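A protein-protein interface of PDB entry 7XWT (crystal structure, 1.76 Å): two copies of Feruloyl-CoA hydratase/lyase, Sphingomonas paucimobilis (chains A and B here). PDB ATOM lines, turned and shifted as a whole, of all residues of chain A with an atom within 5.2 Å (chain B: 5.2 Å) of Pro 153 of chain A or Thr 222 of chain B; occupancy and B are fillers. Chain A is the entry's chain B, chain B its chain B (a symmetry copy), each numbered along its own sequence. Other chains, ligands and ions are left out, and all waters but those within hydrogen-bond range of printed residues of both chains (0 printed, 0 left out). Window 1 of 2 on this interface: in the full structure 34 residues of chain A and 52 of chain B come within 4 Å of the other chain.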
ATOM      1  N   LEU A 144     -21.430 -14.333  10.041  1.00  0.00           N
ATOM      2  CA  LEU A 144     -21.270 -14.302  11.520  1.00  0.00           C
ATOM      3  C   LEU A 144     -22.515 -13.603  12.076  1.00  0.00           C
ATOM      4  O   LEU A 144     -22.506 -12.394  12.385  1.00  0.00           O
ATOM      5  CB  LEU A 144     -19.962 -13.614  11.885  1.00  0.00           C
ATOM      6  CG  LEU A 144     -18.697 -14.346  11.460  1.00  0.00           C
ATOM      7  CD1 LEU A 144     -17.479 -13.558  11.909  1.00  0.00           C
ATOM      8  CD2 LEU A 144     -18.644 -15.765  12.024  1.00  0.00           C
ATOM      9  N   GLU A 146     -23.917 -14.176  14.771  1.00  0.00           N
ATOM     10  CA  GLU A 146     -23.861 -14.134  16.257  1.00  0.00           C
ATOM     11  C   GLU A 146     -24.289 -12.750  16.776  1.00  0.00           C
ATOM     12  O   GLU A 146     -25.115 -12.703  17.705  1.00  0.00           O
ATOM     13  CB  GLU A 146     -22.477 -14.572  16.740  1.00  0.00           C
ATOM     14  CG  GLU A 146     -22.159 -16.058  16.503  1.00  0.00           C
ATOM     15  CD  GLU A 146     -21.267 -16.358  15.290  1.00  0.00           C
ATOM     16  OE1 GLU A 146     -20.418 -17.296  15.352  1.00  0.00           O
ATOM     17  OE2 GLU A 146     -21.415 -15.658  14.271  1.00  0.00           O
ATOM     18  N   VAL A 147     -23.774 -11.637  16.235  1.00  0.00           N
ATOM     19  CA  VAL A 147     -24.062 -10.276  16.774  1.00  0.00           C
ATOM     20  C   VAL A 147     -25.585 -10.032  16.700  1.00  0.00           C
ATOM     21  O   VAL A 147     -26.094  -9.388  17.602  1.00  0.00           O
ATOM     22  CB  VAL A 147     -23.268  -9.169  16.055  1.00  0.00           C
ATOM     23  CG1 VAL A 147     -23.717  -8.969  14.611  1.00  0.00           C
ATOM     24  CG2 VAL A 147     -23.317  -7.855  16.821  1.00  0.00           C
ATOM     25  N   ILE A 151     -24.783 -12.467  20.841  1.00  0.00           N
ATOM     26  CA  ILE A 151     -23.551 -13.162  21.338  1.00  0.00           C
ATOM     27  C   ILE A 151     -22.345 -12.777  20.462  1.00  0.00           C
ATOM     28  O   ILE A 151     -22.508 -12.336  19.310  1.00  0.00           O
ATOM     29  CB  ILE A 151     -23.712 -14.688  21.413  1.00  0.00           C
ATOM     30  CG1 ILE A 151     -23.973 -15.304  20.031  1.00  0.00           C
ATOM     31  CG2 ILE A 151     -24.772 -15.041  22.433  1.00  0.00           C
ATOM     32  CD1 ILE A 151     -23.390 -16.695  19.863  1.00  0.00           C
ATOM     33  N   LEU A 152     -21.142 -12.954  20.991  1.00  0.00           N
ATOM     34  CA  LEU A 152     -19.948 -12.731  20.139  1.00  0.00           C
ATOM     35  C   LEU A 152     -19.688 -14.035  19.360  1.00  0.00           C
ATOM     36  O   LEU A 152     -20.254 -15.089  19.702  1.00  0.00           O
ATOM     37  CB  LEU A 152     -18.784 -12.214  21.006  1.00  0.00           C
ATOM     38  CG  LEU A 152     -18.211 -13.217  21.986  1.00  0.00           C
ATOM     39  CD1 LEU A 152     -17.108 -14.023  21.329  1.00  0.00           C
ATOM     40  CD2 LEU A 152     -17.662 -12.536  23.194  1.00  0.00           C
ATOM     41  N   PRO A 153     -18.937 -13.984  18.231  1.00  0.00           N
ATOM     42  CA  PRO A 153     -18.700 -15.162  17.386  1.00  0.00           C
ATOM     43  C   PRO A 153     -17.686 -16.130  18.035  1.00  0.00           C
ATOM     44  O   PRO A 153     -16.446 -16.060  17.801  1.00  0.00           O
ATOM     45  CB  PRO A 153     -18.254 -14.559  16.044  1.00  0.00           C
ATOM     46  CG  PRO A 153     -18.585 -13.078  16.164  1.00  0.00           C
ATOM     47  CD  PRO A 153     -18.328 -12.792  17.641  1.00  0.00           C
ATOM     48  N   GLY A 154     -18.233 -17.031  18.847  1.00  0.00           N
ATOM     49  CA  GLY A 154     -17.465 -18.091  19.524  1.00  0.00           C
ATOM     50  C   GLY A 154     -17.363 -19.339  18.651  1.00  0.00           C
ATOM     51  O   GLY A 154     -17.561 -19.251  17.367  1.00  0.00           O
ATOM     52  N   GLY A 155     -17.099 -20.477  19.299  1.00  0.00           N
ATOM     53  CA  GLY A 155     -16.681 -21.699  18.592  1.00  0.00           C
ATOM     54  C   GLY A 155     -15.575 -21.366  17.601  1.00  0.00           C
ATOM     55  O   GLY A 155     -15.475 -22.048  16.586  1.00  0.00           O
ATOM     56  N   GLY A 156     -14.715 -20.404  17.958  1.00  0.00           N
ATOM     57  CA  GLY A 156     -13.556 -19.980  17.167  1.00  0.00           C
ATOM     58  C   GLY A 156     -13.938 -19.118  15.988  1.00  0.00           C
ATOM     59  O   GLY A 156     -13.032 -18.741  15.256  1.00  0.00           O
ATOM     60  N   ALA A 157     -15.222 -18.869  15.748  1.00  0.00           N
ATOM     61  CA  ALA A 157     -15.637 -18.267  14.461  1.00  0.00           C
ATOM     62  C   ALA A 157     -14.903 -16.938  14.202  1.00  0.00           C
ATOM     63  O   ALA A 157     -14.637 -16.647  13.031  1.00  0.00           O
ATOM     64  CB  ALA A 157     -17.120 -18.094  14.452  1.00  0.00           C
ATOM     65  N   THR A 158     -14.692 -16.101  15.226  1.00  0.00           N
ATOM     66  CA  THR A 158     -13.985 -14.803  15.124  1.00  0.00           C
ATOM     67  C   THR A 158     -12.562 -15.070  14.555  1.00  0.00           C
ATOM     68  O   THR A 158     -12.104 -14.340  13.673  1.00  0.00           O
ATOM     69  CB  THR A 158     -13.952 -14.022  16.452  1.00  0.00           C
ATOM     70  OG1 THR A 158     -15.256 -13.755  16.980  1.00  0.00           O
ATOM     71  CG2 THR A 158     -13.226 -12.700  16.287  1.00  0.00           C
ATOM     72  N   ALA A 174     -18.044  -9.505  11.491  1.00  0.00           N
ATOM     73  CA  ALA A 174     -18.405  -9.818  12.868  1.00  0.00           C
ATOM     74  C   ALA A 174     -19.296  -8.734  13.508  1.00  0.00           C
ATOM     75  O   ALA A 174     -20.097  -9.095  14.352  1.00  0.00           O
ATOM     76  CB  ALA A 174     -17.146  -9.975  13.664  1.00  0.00           C
ATOM     77  N   MET A 175     -19.077  -7.450  13.221  1.00  0.00           N
ATOM     78  CA  MET A 175     -19.801  -6.338  13.871  1.00  0.00           C
ATOM     79  C   MET A 175     -21.179  -6.155  13.224  1.00  0.00           C
ATOM     80  O   MET A 175     -22.122  -5.839  13.952  1.00  0.00           O
ATOM     81  CB  MET A 175     -19.027  -5.020  13.769  1.00  0.00           C
ATOM     82  CG  MET A 175     -17.727  -4.980  14.547  1.00  0.00           C
ATOM     83  SD  MET A 175     -16.791  -3.455  14.155  1.00  0.00           S
ATOM     84  CE  MET A 175     -17.812  -2.252  14.977  1.00  0.00           C
ATOM     85  N   ALA B 217     -23.127  -3.817  23.936  1.00  0.00           N
ATOM     86  CA  ALA B 217     -22.165  -4.617  24.722  1.00  0.00           C
ATOM     87  C   ALA B 217     -21.609  -5.729  23.827  1.00  0.00           C
ATOM     88  O   ALA B 217     -20.393  -5.945  23.810  1.00  0.00           O
ATOM     89  CB  ALA B 217     -22.834  -5.183  25.945  1.00  0.00           C
ATOM     90  N   THR B 218     -22.487  -6.354  23.050  1.00  0.00           N
ATOM     91  CA  THR B 218     -22.129  -7.394  22.080  1.00  0.00           C
ATOM     92  C   THR B 218     -21.150  -6.807  21.068  1.00  0.00           C
ATOM     93  O   THR B 218     -20.151  -7.505  20.786  1.00  0.00           O
ATOM     94  CB  THR B 218     -23.353  -7.995  21.392  1.00  0.00           C
ATOM     95  OG1 THR B 218     -24.281  -8.368  22.417  1.00  0.00           O
ATOM     96  CG2 THR B 218     -22.956  -9.154  20.496  1.00  0.00           C
ATOM     97  N   VAL B 219     -21.453  -5.623  20.489  1.00  0.00           N
ATOM     98  CA  VAL B 219     -20.550  -4.969  19.500  1.00  0.00           C
ATOM     99  C   VAL B 219     -19.171  -4.676  20.120  1.00  0.00           C
ATOM    100  O   VAL B 219     -18.162  -4.987  19.469  1.00  0.00           O
ATOM    101  CB  VAL B 219     -21.176  -3.741  18.829  1.00  0.00           C
ATOM    102  CG1 VAL B 219     -20.186  -3.026  17.928  1.00  0.00           C
ATOM    103  CG2 VAL B 219     -22.376  -4.194  18.022  1.00  0.00           C
ATOM    104  N   LYS B 220     -19.112  -4.231  21.365  1.00  0.00           N
ATOM    105  CA  LYS B 220     -17.823  -3.898  21.992  1.00  0.00           C
ATOM    106  C   LYS B 220     -17.010  -5.200  22.120  1.00  0.00           C
ATOM    107  O   LYS B 220     -15.796  -5.216  21.761  1.00  0.00           O
ATOM    108  CB  LYS B 220     -18.049  -3.252  23.355  1.00  0.00           C
ATOM    109  CG  LYS B 220     -16.784  -3.113  24.208  1.00  0.00           C
ATOM    110  CD  LYS B 220     -15.586  -2.475  23.503  1.00  0.00           C
ATOM    111  CE  LYS B 220     -14.388  -2.291  24.435  1.00  0.00           C
ATOM    112  NZ  LYS B 220     -13.241  -1.685  23.690  1.00  0.00           N
ATOM    113  N   TYR B 221     -17.609  -6.248  22.665  1.00  0.00           N
ATOM    114  CA  TYR B 221     -16.902  -7.519  22.936  1.00  0.00           C
ATOM    115  C   TYR B 221     -16.431  -8.117  21.621  1.00  0.00           C
ATOM    116  O   TYR B 221     -15.313  -8.578  21.596  1.00  0.00           O
ATOM    117  CB  TYR B 221     -17.733  -8.507  23.739  1.00  0.00           C
ATOM    118  CG  TYR B 221     -17.563  -8.339  25.210  1.00  0.00           C
ATOM    119  CD1 TYR B 221     -18.279  -7.393  25.917  1.00  0.00           C
ATOM    120  CD2 TYR B 221     -16.693  -9.156  25.889  1.00  0.00           C
ATOM    121  CE1 TYR B 221     -18.067  -7.215  27.279  1.00  0.00           C
ATOM    122  CE2 TYR B 221     -16.489  -9.010  27.242  1.00  0.00           C
ATOM    123  CZ  TYR B 221     -17.171  -8.038  27.940  1.00  0.00           C
ATOM    124  OH  TYR B 221     -16.943  -7.941  29.280  1.00  0.00           O
ATOM    125  N   THR B 222     -17.187  -7.947  20.544  1.00  0.00           N
ATOM    126  CA  THR B 222     -16.907  -8.576  19.252  1.00  0.00           C
ATOM    127  C   THR B 222     -15.739  -7.871  18.588  1.00  0.00           C
ATOM    128  O   THR B 222     -14.840  -8.544  18.090  1.00  0.00           O
ATOM    129  CB  THR B 222     -18.122  -8.510  18.306  1.00  0.00           C
ATOM    130  OG1 THR B 222     -19.088  -9.445  18.756  1.00  0.00           O
ATOM    131  CG2 THR B 222     -17.787  -8.914  16.898  1.00  0.00           C
ATOM    132  N   LYS B 223     -15.781  -6.542  18.568  1.00  0.00           N
ATOM    133  CA  LYS B 223     -14.794  -5.711  17.871  1.00  0.00           C
ATOM    134  C   LYS B 223     -13.453  -5.902  18.588  1.00  0.00           C
ATOM    135  O   LYS B 223     -12.444  -6.093  17.911  1.00  0.00           O
ATOM    136  CB  LYS B 223     -15.296  -4.279  17.771  1.00  0.00           C
ATOM    137  CG  LYS B 223     -15.048  -3.369  18.937  1.00  0.00           C
ATOM    138  CD  LYS B 223     -15.990  -2.215  18.921  1.00  0.00           C
ATOM    139  CE  LYS B 223     -15.565  -1.157  19.907  1.00  0.00           C
ATOM    140  NZ  LYS B 223     -14.382  -0.412  19.425  1.00  0.00           N
ATOM    141  N   ASP B 224     -13.472  -5.984  19.903  1.00  0.00           N
ATOM    142  CA  ASP B 224     -12.225  -6.255  20.635  1.00  0.00           C
ATOM    143  C   ASP B 224     -11.727  -7.664  20.297  1.00  0.00           C
ATOM    144  O   ASP B 224     -10.494  -7.850  20.193  1.00  0.00           O
ATOM    145  CB  ASP B 224     -12.393  -6.130  22.139  1.00  0.00           C
ATOM    146  CG  ASP B 224     -12.279  -4.698  22.656  1.00  0.00           C
ATOM    147  OD1 ASP B 224     -12.470  -3.725  21.872  1.00  0.00           O
ATOM    148  OD2 ASP B 224     -11.997  -4.563  23.855  1.00  0.00           O
ATOM    149  N   ALA B 225     -12.625  -8.640  20.189  1.00  0.00           N
ATOM    150  CA  ALA B 225     -12.254 -10.041  19.906  1.00  0.00           C
ATOM    151  C   ALA B 225     -11.510 -10.081  18.575  1.00  0.00           C
ATOM    152  O   ALA B 225     -10.483 -10.739  18.500  1.00  0.00           O
ATOM    153  CB  ALA B 225     -13.474 -10.944  19.903  1.00  0.00           C
ATOM    154  N   VAL B 226     -12.063  -9.465  17.542  1.00  0.00           N
ATOM    155  CA  VAL B 226     -11.388  -9.410  16.236  1.00  0.00           C
ATOM    156  C   VAL B 226      -9.954  -8.879  16.369  1.00  0.00           C
ATOM    157  O   VAL B 226      -9.049  -9.482  15.746  1.00  0.00           O
ATOM    158  CB  VAL B 226     -12.212  -8.597  15.231  1.00  0.00           C
ATOM    159  CG1 VAL B 226     -11.409  -8.340  13.979  1.00  0.00           C
ATOM    160  CG2 VAL B 226     -13.513  -9.314  14.950  1.00  0.00           C
ATOM    161  N   LEU B 241     -12.097 -16.880  23.313  1.00  0.00           N
ATOM    162  CA  LEU B 241     -13.454 -16.454  22.926  1.00  0.00           C
ATOM    163  C   LEU B 241     -14.531 -16.959  23.932  1.00  0.00           C
ATOM    164  O   LEU B 241     -15.543 -16.272  24.114  1.00  0.00           O
ATOM    165  CB  LEU B 241     -13.722 -16.923  21.510  1.00  0.00           C
ATOM    166  CG  LEU B 241     -12.886 -16.194  20.459  1.00  0.00           C
ATOM    167  CD1 LEU B 241     -12.883 -16.964  19.149  1.00  0.00           C
ATOM    168  CD2 LEU B 241     -13.402 -14.798  20.241  1.00  0.00           C
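Of the 13 printed residues of chain A, 8 touch a printed residue of chain B.
Hydrophobic or aromatic side chains of chain A that line the printed part of chain B: Val 147, Leu 152, Pro 153, Ala 174 and Met 175.
Of the 11 printed residues of chain B, 7 touch a printed residue of chain A.
Printed residues of chain B that touch a printed residue of chain A: Thr 218, Val 219, Thr 222, Lys 223, Ala 225, Val 226 and Leu 241.
Among the printed residues, 15 pairs touch across the chains.
Leu 144 of chain A touches none of the printed residues of chain B.
Of the printed residues of chain B, Val 147 of chain A touches Thr 218 (3.9 Å) and Val 219 (3.97 Å).
Of chain B, only Thr 222 (3.6 Å) and Leu 241 (3.9 Å) come within 4 Å of Pro 153 of chain A.
Of the printed residues of chain B, Ala 174 of chain A touches Thr 222 and Val 226.
Printed residues of chain B within 4 Å of Met 175 of chain A: Val 219 (3.9 Å) and Lys 223 (3.999 Å).
Val 147 of chain A touches Thr 218 of chain B.
CG2 of Thr 218 of chain B touches O of Ile 151 of chain A (3.4 Å).
Thr 222 of chain B touches Pro 153 of chain A.
CD1 of Leu 241 of chain B touches CA of Gly 156 of chain A (3.7 Å).
Thr 158 of chain A touches Ala 225 of chain B.
Thr 158 of chain A touches Val 226 of chain B.
OG1 of Thr 158 of chain A touches CD2 of Leu 241 of chain B (3.9 Å).
O of Ala 174 of chain A touches CG2 of Thr 222 of chain B, at 3.4 Å.
Val 219 of chain B touches Met 175 of chain A (CG1 to CE, 3.9 Å).
Met 175 of chain A touches Lys 223 of chain B (SD to CB, 3.999 Å).
OG1 of Thr 222 of chain B sits at hydrogen-bond distance from O of Thr 218 of chain B.
The backbone carbonyl oxygen (O) of Glu 146 of chain A is in hydrogen-bond range of the backbone NH (N) of Ile 151 of chain A.
The backbone carbonyl oxygen of Pro 153 of chain A lies within hydrogen-bond range of the side-chain hydroxyl of Thr 158 of chain A (2.7 Å).
No position is printed for both chains.
Of the 15 pairs that touch across the chains among the printed residues, none has its exchanged pair printed and touching as well.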
